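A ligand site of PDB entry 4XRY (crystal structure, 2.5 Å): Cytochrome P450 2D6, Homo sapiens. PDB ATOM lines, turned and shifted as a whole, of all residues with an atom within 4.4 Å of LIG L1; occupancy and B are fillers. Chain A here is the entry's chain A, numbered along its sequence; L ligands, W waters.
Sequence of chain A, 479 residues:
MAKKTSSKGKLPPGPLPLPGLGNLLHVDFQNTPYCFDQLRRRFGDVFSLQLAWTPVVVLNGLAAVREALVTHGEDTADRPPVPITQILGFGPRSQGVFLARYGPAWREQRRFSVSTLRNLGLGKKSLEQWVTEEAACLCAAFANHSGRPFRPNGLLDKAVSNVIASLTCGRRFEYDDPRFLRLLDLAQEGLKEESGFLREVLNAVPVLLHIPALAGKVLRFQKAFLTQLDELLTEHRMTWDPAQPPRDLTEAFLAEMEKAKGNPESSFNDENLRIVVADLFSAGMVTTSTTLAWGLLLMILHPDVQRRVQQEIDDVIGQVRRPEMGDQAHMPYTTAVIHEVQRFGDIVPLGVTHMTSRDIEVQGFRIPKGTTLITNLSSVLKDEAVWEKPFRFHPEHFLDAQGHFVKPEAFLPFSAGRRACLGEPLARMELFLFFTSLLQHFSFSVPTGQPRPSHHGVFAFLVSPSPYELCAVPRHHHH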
ATOM      1  N   ARG A  79     -15.520  30.663   1.753  1.00  0.00           N
ATOM      2  CA  ARG A  79     -14.649  31.444   2.636  1.00  0.00           C
ATOM      3  C   ARG A  79     -15.499  32.321   3.548  1.00  0.00           C
ATOM      4  O   ARG A  79     -16.584  32.746   3.156  1.00  0.00           O
ATOM      5  CB  ARG A  79     -13.689  32.324   1.829  1.00  0.00           C
ATOM      6  CG  ARG A  79     -12.722  31.572   0.930  1.00  0.00           C
ATOM      7  CD  ARG A  79     -11.578  30.963   1.723  1.00  0.00           C
ATOM      8  NE  ARG A  79     -10.570  30.406   0.823  1.00  0.00           N
ATOM      9  CZ  ARG A  79      -9.905  29.275   1.039  1.00  0.00           C
ATOM     10  NH1 ARG A  79      -9.015  28.852   0.152  1.00  0.00           N
ATOM     11  NH2 ARG A  79     -10.134  28.553   2.136  1.00  0.00           N
ATOM     12  N   VAL A  97      -9.186  34.726  -6.312  1.00  0.00           N
ATOM     13  CA  VAL A  97      -9.416  33.303  -6.119  1.00  0.00           C
ATOM     14  C   VAL A  97      -9.313  32.938  -4.656  1.00  0.00           C
ATOM     15  O   VAL A  97     -10.164  32.227  -4.120  1.00  0.00           O
ATOM     16  CB  VAL A  97      -8.408  32.450  -6.914  1.00  0.00           C
ATOM     17  CG1 VAL A  97      -8.659  30.969  -6.682  1.00  0.00           C
ATOM     18  CG2 VAL A  97      -8.484  32.763  -8.396  1.00  0.00           C
ATOM     19  N   PHE A  98      -8.273  33.452  -4.015  1.00  0.00           N
ATOM     20  CA  PHE A  98      -7.909  33.073  -2.653  1.00  0.00           C
ATOM     21  C   PHE A  98      -9.029  33.312  -1.643  1.00  0.00           C
ATOM     22  O   PHE A  98      -9.423  32.407  -0.917  1.00  0.00           O
ATOM     23  CB  PHE A  98      -6.653  33.824  -2.221  1.00  0.00           C
ATOM     24  CG  PHE A  98      -5.964  33.218  -1.034  1.00  0.00           C
ATOM     25  CD1 PHE A  98      -5.033  32.204  -1.193  1.00  0.00           C
ATOM     26  CD2 PHE A  98      -6.252  33.660   0.253  1.00  0.00           C
ATOM     27  CE1 PHE A  98      -4.391  31.644  -0.107  1.00  0.00           C
ATOM     28  CE2 PHE A  98      -5.619  33.100   1.354  1.00  0.00           C
ATOM     29  CZ  PHE A  98      -4.686  32.098   1.175  1.00  0.00           C
ATOM     30  N   TRP A 106     -15.508  32.679  -8.099  1.00  0.00           N
ATOM     31  CA  TRP A 106     -14.391  31.845  -7.682  1.00  0.00           C
ATOM     32  C   TRP A 106     -14.091  30.743  -8.700  1.00  0.00           C
ATOM     33  O   TRP A 106     -12.933  30.529  -9.058  1.00  0.00           O
ATOM     34  CB  TRP A 106     -14.650  31.206  -6.316  1.00  0.00           C
ATOM     35  CG  TRP A 106     -13.706  30.083  -6.006  1.00  0.00           C
ATOM     36  CD1 TRP A 106     -12.443  30.190  -5.490  1.00  0.00           C
ATOM     37  CD2 TRP A 106     -13.931  28.682  -6.222  1.00  0.00           C
ATOM     38  NE1 TRP A 106     -11.882  28.941  -5.356  1.00  0.00           N
ATOM     39  CE2 TRP A 106     -12.782  27.998  -5.800  1.00  0.00           C
ATOM     40  CE3 TRP A 106     -15.018  27.943  -6.726  1.00  0.00           C
ATOM     41  CZ2 TRP A 106     -12.667  26.608  -5.874  1.00  0.00           C
ATOM     42  CZ3 TRP A 106     -14.898  26.566  -6.796  1.00  0.00           C
ATOM     43  CH2 TRP A 106     -13.730  25.912  -6.367  1.00  0.00           C
ATOM     44  N   ARG A 110     -10.788  30.164 -10.719  1.00  0.00           N
ATOM     45  CA  ARG A 110     -10.130  28.930 -10.329  1.00  0.00           C
ATOM     46  C   ARG A 110      -9.827  28.056 -11.548  1.00  0.00           C
ATOM     47  O   ARG A 110      -8.715  27.601 -11.741  1.00  0.00           O
ATOM     48  CB  ARG A 110     -10.977  28.151  -9.315  1.00  0.00           C
ATOM     49  CG  ARG A 110     -10.500  26.727  -9.034  1.00  0.00           C
ATOM     50  CD  ARG A 110      -9.605  26.650  -7.809  1.00  0.00           C
ATOM     51  NE  ARG A 110      -9.094  25.297  -7.601  1.00  0.00           N
ATOM     52  CZ  ARG A 110      -8.352  24.924  -6.560  1.00  0.00           C
ATOM     53  NH1 ARG A 110      -8.034  25.804  -5.628  1.00  0.00           N
ATOM     54  NH2 ARG A 110      -7.927  23.667  -6.465  1.00  0.00           N
ATOM     55  N   ILE A 164       6.874  33.218 -10.589  1.00  0.00           N
ATOM     56  CA  ILE A 164       5.493  33.635 -10.674  1.00  0.00           C
ATOM     57  C   ILE A 164       5.342  34.775 -11.671  1.00  0.00           C
ATOM     58  O   ILE A 164       4.417  34.770 -12.491  1.00  0.00           O
ATOM     59  CB  ILE A 164       4.954  34.087  -9.314  1.00  0.00           C
ATOM     60  CG1 ILE A 164       5.332  33.071  -8.227  1.00  0.00           C
ATOM     61  CG2 ILE A 164       3.454  34.240  -9.389  1.00  0.00           C
ATOM     62  CD1 ILE A 164       4.630  31.739  -8.364  1.00  0.00           C
ATOM     63  N   LEU A 280      -2.033  35.271  -6.913  1.00  0.00           N
ATOM     64  CA  LEU A 280      -1.079  34.309  -7.476  1.00  0.00           C
ATOM     65  C   LEU A 280       0.349  34.671  -7.112  1.00  0.00           C
ATOM     66  O   LEU A 280       1.135  33.813  -6.700  1.00  0.00           O
ATOM     67  CB  LEU A 280      -1.221  34.234  -8.993  1.00  0.00           C
ATOM     68  CG  LEU A 280      -2.474  33.562  -9.540  1.00  0.00           C
ATOM     69  CD1 LEU A 280      -2.498  33.670 -11.054  1.00  0.00           C
ATOM     70  CD2 LEU A 280      -2.525  32.108  -9.091  1.00  0.00           C
ATOM     71  N   ALA A 283       0.759  34.379  -2.924  1.00  0.00           N
ATOM     72  CA  ALA A 283       0.472  33.074  -2.304  1.00  0.00           C
ATOM     73  C   ALA A 283       1.545  32.043  -2.618  1.00  0.00           C
ATOM     74  O   ALA A 283       1.779  31.129  -1.838  1.00  0.00           O
ATOM     75  CB  ALA A 283      -0.892  32.560  -2.740  1.00  0.00           C
ATOM     76  N   GLY A 284       2.203  32.204  -3.767  1.00  0.00           N
ATOM     77  CA  GLY A 284       3.263  31.305  -4.169  1.00  0.00           C
ATOM     78  C   GLY A 284       4.614  31.979  -4.138  1.00  0.00           C
ATOM     79  O   GLY A 284       5.473  31.723  -4.991  1.00  0.00           O
ATOM     80  N   THR A 287       5.189  31.131   0.492  1.00  0.00           N
ATOM     81  CA  THR A 287       5.023  29.721   0.827  1.00  0.00           C
ATOM     82  C   THR A 287       6.175  28.879   0.272  1.00  0.00           C
ATOM     83  O   THR A 287       6.834  28.167   1.021  1.00  0.00           O
ATOM     84  CB  THR A 287       3.686  29.162   0.297  1.00  0.00           C
ATOM     85  OG1 THR A 287       3.511  29.572  -1.068  1.00  0.00           O
ATOM     86  CG2 THR A 287       2.525  29.676   1.138  1.00  0.00           C
ATOM     87  N   THR A 288       6.390  28.963  -1.036  1.00  0.00           N
ATOM     88  CA  THR A 288       7.444  28.199  -1.686  1.00  0.00           C
ATOM     89  C   THR A 288       8.836  28.591  -1.185  1.00  0.00           C
ATOM     90  O   THR A 288       9.718  27.737  -1.050  1.00  0.00           O
ATOM     91  CB  THR A 288       7.389  28.361  -3.213  1.00  0.00           C
ATOM     92  OG1 THR A 288       6.049  28.156  -3.666  1.00  0.00           O
ATOM     93  CG2 THR A 288       8.313  27.369  -3.903  1.00  0.00           C
ATOM     94  N   THR A 291       9.392  27.324   2.423  1.00  0.00           N
ATOM     95  CA  THR A 291       9.632  25.890   2.337  1.00  0.00           C
ATOM     96  C   THR A 291      11.081  25.606   1.981  1.00  0.00           C
ATOM     97  O   THR A 291      11.723  24.754   2.588  1.00  0.00           O
ATOM     98  CB  THR A 291       8.700  25.215   1.303  1.00  0.00           C
ATOM     99  OG1 THR A 291       7.338  25.352   1.729  1.00  0.00           O
ATOM    100  CG2 THR A 291       9.035  23.748   1.183  1.00  0.00           C
ATOM    101  N   GLN A 342       8.467  19.620   3.696  1.00  0.00           N
ATOM    102  CA  GLN A 342       7.125  20.183   3.782  1.00  0.00           C
ATOM    103  C   GLN A 342       6.411  19.684   5.037  1.00  0.00           C
ATOM    104  O   GLN A 342       5.751  20.449   5.740  1.00  0.00           O
ATOM    105  CB  GLN A 342       6.303  19.831   2.540  1.00  0.00           C
ATOM    106  CG  GLN A 342       6.854  20.389   1.238  1.00  0.00           C
ATOM    107  CD  GLN A 342       5.812  20.445   0.142  1.00  0.00           C
ATOM    108  OE1 GLN A 342       5.716  19.532  -0.694  1.00  0.00           O
ATOM    109  NE2 GLN A 342       5.017  21.514   0.123  1.00  0.00           N
ATOM    110  N   ILE A 347       4.400  24.683   7.267  1.00  0.00           N
ATOM    111  CA  ILE A 347       4.439  26.143   7.196  1.00  0.00           C
ATOM    112  C   ILE A 347       3.087  26.840   7.238  1.00  0.00           C
ATOM    113  O   ILE A 347       3.027  28.039   7.498  1.00  0.00           O
ATOM    114  CB  ILE A 347       5.184  26.603   5.927  1.00  0.00           C
ATOM    115  CG1 ILE A 347       4.327  26.358   4.684  1.00  0.00           C
ATOM    116  CG2 ILE A 347       6.526  25.891   5.814  1.00  0.00           C
ATOM    117  CD1 ILE A 347       4.996  26.767   3.396  1.00  0.00           C
ATOM    118  N   VAL A 348       2.002  26.104   6.995  1.00  0.00           N
ATOM    119  CA  VAL A 348       0.658  26.646   7.185  1.00  0.00           C
ATOM    120  C   VAL A 348      -0.110  25.757   8.152  1.00  0.00           C
ATOM    121  O   VAL A 348      -1.005  25.021   7.745  1.00  0.00           O
ATOM    122  CB  VAL A 348      -0.124  26.749   5.856  1.00  0.00           C
ATOM    123  CG1 VAL A 348      -1.115  27.899   5.922  1.00  0.00           C
ATOM    124  CG2 VAL A 348       0.806  26.933   4.686  1.00  0.00           C
ATOM    125  N   VAL A 352      -5.919  27.645   5.605  1.00  0.00           N
ATOM    126  CA  VAL A 352      -6.694  28.839   5.316  1.00  0.00           C
ATOM    127  C   VAL A 352      -8.140  28.559   5.700  1.00  0.00           C
ATOM    128  O   VAL A 352      -8.655  27.484   5.405  1.00  0.00           O
ATOM    129  CB  VAL A 352      -6.576  29.259   3.838  1.00  0.00           C
ATOM    130  CG1 VAL A 352      -7.415  30.484   3.547  1.00  0.00           C
ATOM    131  CG2 VAL A 352      -5.128  29.520   3.490  1.00  0.00           C
ATOM    132  N   HIS A 354     -12.034  27.986   6.211  1.00  0.00           N
ATOM    133  CA  HIS A 354     -13.184  27.679   5.374  1.00  0.00           C
ATOM    134  C   HIS A 354     -14.450  28.111   6.092  1.00  0.00           C
ATOM    135  O   HIS A 354     -14.416  28.507   7.257  1.00  0.00           O
ATOM    136  CB  HIS A 354     -13.244  26.185   5.045  1.00  0.00           C
ATOM    137  CG  HIS A 354     -12.136  25.719   4.161  1.00  0.00           C
ATOM    138  ND1 HIS A 354     -12.358  25.057   2.971  1.00  0.00           N
ATOM    139  CD2 HIS A 354     -10.790  25.813   4.285  1.00  0.00           C
ATOM    140  CE1 HIS A 354     -11.212  24.767   2.406  1.00  0.00           C
ATOM    141  NE2 HIS A 354     -10.234  25.209   3.184  1.00  0.00           N
ATOM    142  N   LEU A 377      -4.015  21.635   9.711  1.00  0.00           N
ATOM    143  CA  LEU A 377      -3.155  20.834   8.849  1.00  0.00           C
ATOM    144  C   LEU A 377      -1.954  20.282   9.613  1.00  0.00           C
ATOM    145  O   LEU A 377      -1.458  19.200   9.306  1.00  0.00           O
ATOM    146  CB  LEU A 377      -2.675  21.663   7.647  1.00  0.00           C
ATOM    147  CG  LEU A 377      -3.779  22.219   6.741  1.00  0.00           C
ATOM    148  CD1 LEU A 377      -3.164  23.000   5.588  1.00  0.00           C
ATOM    149  CD2 LEU A 377      -4.675  21.110   6.217  1.00  0.00           C
ATOM    150  N   PRO A 413      -0.003  19.017   3.030  1.00  0.00           N
ATOM    151  CA  PRO A 413       0.411  20.410   3.250  1.00  0.00           C
ATOM    152  C   PRO A 413      -0.323  21.397   2.345  1.00  0.00           C
ATOM    153  O   PRO A 413      -0.370  22.583   2.662  1.00  0.00           O
ATOM    154  CB  PRO A 413       1.906  20.381   2.926  1.00  0.00           C
ATOM    155  CG  PRO A 413       2.028  19.309   1.899  1.00  0.00           C
ATOM    156  CD  PRO A 413       1.002  18.259   2.263  1.00  0.00           C
ATOM    157  N   PHE A 414      -0.900  20.918   1.253  1.00  0.00           N
ATOM    158  CA  PHE A 414      -1.653  21.773   0.345  1.00  0.00           C
ATOM    159  C   PHE A 414      -3.142  21.719   0.621  1.00  0.00           C
ATOM    160  O   PHE A 414      -3.947  22.142  -0.209  1.00  0.00           O
ATOM    161  CB  PHE A 414      -1.395  21.376  -1.116  1.00  0.00           C
ATOM    162  CG  PHE A 414       0.040  21.483  -1.534  1.00  0.00           C
ATOM    163  CD1 PHE A 414       0.830  20.352  -1.674  1.00  0.00           C
ATOM    164  CD2 PHE A 414       0.605  22.723  -1.796  1.00  0.00           C
ATOM    165  CE1 PHE A 414       2.149  20.446  -2.060  1.00  0.00           C
ATOM    166  CE2 PHE A 414       1.929  22.825  -2.192  1.00  0.00           C
ATOM    167  CZ  PHE A 414       2.701  21.689  -2.317  1.00  0.00           C
ATOM    168  N   SER A 415      -3.501  21.206   1.790  1.00  0.00           N
ATOM    169  CA  SER A 415      -4.900  20.966   2.187  1.00  0.00           C
ATOM    170  C   SER A 415      -5.551  19.944   1.259  1.00  0.00           C
ATOM    171  O   SER A 415      -4.873  19.087   0.692  1.00  0.00           O
ATOM    172  CB  SER A 415      -5.703  22.265   2.196  1.00  0.00           C
ATOM    173  OG  SER A 415      -7.011  22.044   2.684  1.00  0.00           O
ATOM    174  N   ARG A 419     -10.946  23.509  -2.630  1.00  0.00           N
ATOM    175  CA  ARG A 419     -10.142  24.697  -2.371  1.00  0.00           C
ATOM    176  C   ARG A 419      -8.660  24.390  -2.173  1.00  0.00           C
ATOM    177  O   ARG A 419      -7.880  25.295  -1.875  1.00  0.00           O
ATOM    178  CB  ARG A 419     -10.682  25.441  -1.151  1.00  0.00           C
ATOM    179  CG  ARG A 419     -11.986  26.187  -1.397  1.00  0.00           C
ATOM    180  CD  ARG A 419     -11.742  27.485  -2.153  1.00  0.00           C
ATOM    181  NE  ARG A 419     -12.920  28.344  -2.112  1.00  0.00           N
ATOM    182  CZ  ARG A 419     -12.893  29.669  -2.133  1.00  0.00           C
ATOM    183  NH1 ARG A 419     -11.732  30.316  -2.197  1.00  0.00           N
ATOM    184  NH2 ARG A 419     -14.028  30.347  -2.089  1.00  0.00           N
ATOM    185  N   ALA A 420      -8.279  23.127  -2.325  1.00  0.00           N
ATOM    186  CA  ALA A 420      -6.867  22.747  -2.190  1.00  0.00           C
ATOM    187  C   ALA A 420      -5.999  23.588  -3.118  1.00  0.00           C
ATOM    188  O   ALA A 420      -6.426  23.960  -4.215  1.00  0.00           O
ATOM    189  CB  ALA A 420      -6.691  21.270  -2.476  1.00  0.00           C
ATOM    190  N   CYS A 421      -4.787  23.901  -2.659  1.00  0.00           N
ATOM    191  CA  CYS A 421      -3.842  24.788  -3.357  1.00  0.00           C
ATOM    192  C   CYS A 421      -3.814  24.571  -4.873  1.00  0.00           C
ATOM    193  O   CYS A 421      -3.471  23.488  -5.334  1.00  0.00           O
ATOM    194  CB  CYS A 421      -2.440  24.612  -2.775  1.00  0.00           C
ATOM    195  SG  CYS A 421      -1.189  25.768  -3.394  1.00  0.00           S
ATOM    196  N   LEU A 422      -4.177  25.598  -5.634  1.00  0.00           N
ATOM    197  CA  LEU A 422      -4.184  25.454  -7.087  1.00  0.00           C
ATOM    198  C   LEU A 422      -2.766  25.527  -7.637  1.00  0.00           C
ATOM    199  O   LEU A 422      -2.511  25.131  -8.770  1.00  0.00           O
ATOM    200  CB  LEU A 422      -5.074  26.522  -7.741  1.00  0.00           C
ATOM    201  CG  LEU A 422      -4.750  28.031  -7.782  1.00  0.00           C
ATOM    202  CD1 LEU A 422      -3.707  28.382  -8.842  1.00  0.00           C
ATOM    203  CD2 LEU A 422      -6.030  28.816  -8.032  1.00  0.00           C
ATOM    204  N   GLY A 423      -1.826  26.004  -6.821  1.00  0.00           N
ATOM    205  CA  GLY A 423      -0.457  26.167  -7.240  1.00  0.00           C
ATOM    206  C   GLY A 423       0.442  24.974  -6.978  1.00  0.00           C
ATOM    207  O   GLY A 423       1.630  25.001  -7.315  1.00  0.00           O
ATOM    208  N   LEU A 426       2.951  23.629  -9.706  1.00  0.00           N
ATOM    209  CA  LEU A 426       4.055  24.557  -9.830  1.00  0.00           C
ATOM    210  C   LEU A 426       4.979  24.466  -8.621  1.00  0.00           C
ATOM    211  O   LEU A 426       6.209  24.453  -8.762  1.00  0.00           O
ATOM    212  CB  LEU A 426       3.540  25.990  -9.982  1.00  0.00           C
ATOM    213  CG  LEU A 426       4.621  27.077 -10.034  1.00  0.00           C
ATOM    214  CD1 LEU A 426       5.518  26.876 -11.238  1.00  0.00           C
ATOM    215  CD2 LEU A 426       3.976  28.458 -10.053  1.00  0.00           C
ATOM    216  N   ALA A 427       4.387  24.402  -7.432  1.00  0.00           N
ATOM    217  CA  ALA A 427       5.144  24.286  -6.190  1.00  0.00           C
ATOM    218  C   ALA A 427       6.022  23.038  -6.203  1.00  0.00           C
ATOM    219  O   ALA A 427       7.199  23.088  -5.840  1.00  0.00           O
ATOM    220  CB  ALA A 427       4.205  24.270  -4.993  1.00  0.00           C
ATOM    221  N   GLU A 430       8.876  23.868  -8.540  1.00  0.00           N
ATOM    222  CA  GLU A 430       9.810  24.818  -7.946  1.00  0.00           C
ATOM    223  C   GLU A 430      10.663  24.165  -6.864  1.00  0.00           C
ATOM    224  O   GLU A 430      11.874  24.369  -6.810  1.00  0.00           O
ATOM    225  CB  GLU A 430       9.062  26.015  -7.354  1.00  0.00           C
ATOM    226  CG  GLU A 430       8.518  26.986  -8.395  1.00  0.00           C
ATOM    227  CD  GLU A 430       7.801  28.157  -7.754  1.00  0.00           C
ATOM    228  OE1 GLU A 430       8.207  29.315  -7.988  1.00  0.00           O
ATOM    229  OE2 GLU A 430       6.807  27.928  -7.022  1.00  0.00           O
ATOM    230  N   LEU A 431      10.026  23.374  -6.001  1.00  0.00           N
ATOM    231  CA  LEU A 431      10.725  22.713  -4.907  1.00  0.00           C
ATOM    232  C   LEU A 431      11.776  21.748  -5.423  1.00  0.00           C
ATOM    233  O   LEU A 431      12.933  21.838  -5.037  1.00  0.00           O
ATOM    234  CB  LEU A 431       9.733  21.992  -3.991  1.00  0.00           C
ATOM    235  CG  LEU A 431       8.858  22.923  -3.151  1.00  0.00           C
ATOM    236  CD1 LEU A 431       7.929  22.131  -2.228  1.00  0.00           C
ATOM    237  CD2 LEU A 431       9.715  23.901  -2.363  1.00  0.00           C
HETATM  238  C1  LIG L   1      -4.416  27.694  -1.347  1.00  0.00           C
HETATM  239  C2  LIG L   1      -0.418  25.726   0.623  1.00  0.00           C
HETATM  240  C3  LIG L   1       2.256  27.434  -3.068  1.00  0.00           C
HETATM  241  C4  LIG L   1      -1.672  29.667  -4.827  1.00  0.00           C
HETATM  242  C5  LIG L   1      -3.564  27.051  -0.463  1.00  0.00           C
HETATM  243  C6  LIG L   1      -3.916  26.505   0.836  1.00  0.00           C
HETATM  244  C7  LIG L   1      -2.824  25.967   1.370  1.00  0.00           C
HETATM  245  C8  LIG L   1      -1.727  26.138   0.434  1.00  0.00           C
HETATM  246  C9  LIG L   1      -2.759  25.297   2.721  1.00  0.00           C
HETATM  247  C10 LIG L   1      -5.307  26.548   1.492  1.00  0.00           C
HETATM  248  C11 LIG L   1      -6.257  25.538   0.857  1.00  0.00           C
HETATM  249  C12 LIG L   1      -7.590  25.669   1.541  1.00  0.00           C
HETATM  250  O1  LIG L   1      -8.133  26.793   1.599  1.00  0.00           O
HETATM  251  O2  LIG L   1      -8.117  24.631   2.032  1.00  0.00           O
HETATM  252  C13 LIG L   1       0.654  25.980  -0.216  1.00  0.00           C
HETATM  253  C14 LIG L   1       2.009  25.481  -0.054  1.00  0.00           C
HETATM  254  C15 LIG L   1       2.752  25.949  -1.072  1.00  0.00           C
HETATM  255  C16 LIG L   1       1.889  26.768  -1.902  1.00  0.00           C
HETATM  256  C17 LIG L   1       2.424  24.597   1.097  1.00  0.00           C
HETATM  257  C18 LIG L   1       4.253  25.744  -1.390  1.00  0.00           C
HETATM  258  C19 LIG L   1       5.097  25.002  -0.668  1.00  0.00           C
HETATM  259  C20 LIG L   1       1.412  28.111  -3.918  1.00  0.00           C
HETATM  260  C21 LIG L   1       1.712  28.552  -5.276  1.00  0.00           C
HETATM  261  C22 LIG L   1       0.617  29.170  -5.754  1.00  0.00           C
HETATM  262  C23 LIG L   1      -0.397  29.136  -4.721  1.00  0.00           C
HETATM  263  C24 LIG L   1       3.047  28.316  -5.948  1.00  0.00           C
HETATM  264  C25 LIG L   1       0.357  29.835  -7.135  1.00  0.00           C
HETATM  265  C26 LIG L   1       1.230  29.899  -8.144  1.00  0.00           C
HETATM  266  C27 LIG L   1      -2.757  29.341  -4.048  1.00  0.00           C
HETATM  267  C28 LIG L   1      -4.120  29.814  -4.217  1.00  0.00           C
HETATM  268  C29 LIG L   1      -4.878  29.278  -3.268  1.00  0.00           C
HETATM  269  C30 LIG L   1      -4.025  28.433  -2.445  1.00  0.00           C
HETATM  270  C31 LIG L   1      -4.584  30.758  -5.295  1.00  0.00           C
HETATM  271  C32 LIG L   1      -6.399  29.498  -3.061  1.00  0.00           C
HETATM  272  C33 LIG L   1      -7.166  28.406  -3.812  1.00  0.00           C
HETATM  273  C34 LIG L   1      -8.663  28.563  -3.604  1.00  0.00           C
HETATM  274  O3  LIG L   1      -9.454  27.984  -4.397  1.00  0.00           O
HETATM  275  O4  LIG L   1      -9.074  29.273  -2.654  1.00  0.00           O
HETATM  276  N1  LIG L   1      -2.223  26.803  -0.668  1.00  0.00           N
HETATM  277  N2  LIG L   1       0.620  26.757  -1.353  1.00  0.00           N
HETATM  278  N3  LIG L   1       0.117  28.479  -3.622  1.00  0.00           N
HETATM  279  N4  LIG L   1      -2.748  28.499  -2.952  1.00  0.00           N
HETATM  280 FE1  LIG L   1      -1.062  27.611  -2.165  1.00  0.00          FE
HETATM  281  C1  LG2 L   2      -1.050  38.326   0.965  1.00  0.00           C
HETATM  282  C2  LG2 L   2      -1.970  39.358   0.859  1.00  0.00           C
HETATM  283  C3  LG2 L   2      -1.590  40.664   0.604  1.00  0.00           C
HETATM  284  C4  LG2 L   2      -0.259  40.926   0.463  1.00  0.00           C
HETATM  285  C5  LG2 L   2       0.709  39.951   0.555  1.00  0.00           C
HETATM  286  C6  LG2 L   2       0.288  38.673   0.789  1.00  0.00           C
HETATM  287  F1  LG2 L   2       1.218  37.698   0.848  1.00  0.00           F
HETATM  288  C7  LG2 L   2      -0.789  36.329   2.490  1.00  0.00           C
HETATM  289  O1  LG2 L   2      -1.023  34.929   2.660  1.00  0.00           O
HETATM  290  C8  LG2 L   2      -0.615  34.194   1.531  1.00  0.00           C
HETATM  291  C9  LG2 L   2      -1.564  34.509   0.388  1.00  0.00           C
HETATM  292  C10 LG2 L   2      -0.718  32.767   1.952  1.00  0.00           C
HETATM  293  F2  LG2 L   2       0.140  42.202   0.235  1.00  0.00           F
HETATM  294  C11 LG2 L   2      -1.567  36.902   1.262  1.00  0.00           C
HETATM  295  C12 LG2 L   2      -1.392  35.984   0.009  1.00  0.00           C
HETATM  296  C13 LG2 L   2      -2.318  36.405  -1.122  1.00  0.00           C
HETATM  297  S1  LG2 L   2      -4.082  36.414  -0.731  1.00  0.00           S
HETATM  298  C14 LG2 L   2      -4.010  36.764   1.033  1.00  0.00           C
HETATM  299  N1  LG2 L   2      -2.951  36.950   1.782  1.00  0.00           N
HETATM  300  N2  LG2 L   2      -5.223  36.819   1.580  1.00  0.00           N
HETATM  301  C15 LG2 L   2      -0.447  32.236   3.260  1.00  0.00           C
HETATM  302  N3  LG2 L   2      -0.657  30.932   3.281  1.00  0.00           N
HETATM  303  N4  LG2 L   2      -1.056  30.597   2.000  1.00  0.00           N
HETATM  304  C16 LG2 L   2      -1.102  31.660   1.186  1.00  0.00           C
HETATM  305  C17 LG2 L   2      -1.368  29.210   1.682  1.00  0.00           C
HETATM  306  O   HOH W   1       5.545  23.203   2.129  1.00  0.00           O
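SG of Cys 421 binds FE1 of LIG L1 (2.2 Å).
An oxygen (O2) of LIG L1 is in hydrogen-bond range of a ring nitrogen (NE2) of His 354, 2.5 Å away.
NH1 of Arg 79 is in salt-bridge range of O1 of LIG L1 (2.7 Å).
The indole nitrogen (NE1) of Trp 106 is in hydrogen-bond range of an oxygen (O3) of LIG L1, 2.8 Å away.
An oxygen (O3) of LIG L1 lies within salt-bridge range of the guanidinium group (NH1) of Arg 110.
O2 of LIG L1 is in hydrogen-bond range of OG of Ser 415 (2.9 Å).
An oxygen (O4) of LIG L1 lies within salt-bridge range of the guanidinium group of Arg 419, at 2.9 Å.
N of Cys 421 sits at hydrogen-bond distance from O of Phe 414 (3.1 Å).
The side-chain sulfur (SG) of Cys 421 lies close to the backbone NH (N) of Gly 423 (3.5 Å).
The backbone carbonyl oxygen of Phe 98 is in hydrogen-bond range of the guanidinium group of Arg 79 (2.9 Å).
The guanidinium group (NH1) of Arg 419 is in hydrogen-bond range of the backbone carbonyl oxygen (O) of Val 97.
The guanidinium group (NH1) of Arg 419 lies within hydrogen-bond range of the backbone carbonyl oxygen (O) of Phe 98 (3.4 Å).
OG1 of Thr 291 is in hydrogen-bond range of O of Thr 287, 2.9 Å away.
O of Ala 283 is in hydrogen-bond range of OG1 of Thr 287 (2.5 Å).
The side-chain carboxylate (OE2) of Glu 430 is in hydrogen-bond range of the side-chain hydroxyl (OG1) of Thr 288.
O4 of LIG L1 sits close to O of Val 97 (3.5 Å).
Residues that only touch LIG L1: Phe 98, Ile 164, Ala 283, Gly 284, Thr 287, Thr 288, Thr 291, Gln 342, Val 352, Leu 377, Pro 413, Phe 414, Leu 422, Gly 423, Leu 426, Ala 427 and Glu 430.
Hydrophobic or aromatic side chains that line LIG L1: Val 97, Phe 98, Trp 106, Ile 164, Ala 283, Val 352, His 354, Leu 377, Phe 414, Leu 422, Leu 426 and Ala 427.
Within 4 Å of LIG L1: Arg 79, Val 97, Phe 98, Trp 106, Arg 110, Ile 164, Ala 283, Gly 284, Thr 287, Thr 288, Thr 291, Gln 342, Val 352, His 354, Leu 377, Pro 413, Phe 414, Ser 415, Arg 419, Cys 421, Leu 422, Gly 423, Leu 426, Ala 427 and Glu 430.
The nearest printed residue that does not touch LIG L1 is Ile 347 (4.1 Å).
Water W1 bridges the side-chain amide nitrogen (NE2) of Gln 342 and the side-chain hydroxyl (OG1) of Thr 291.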
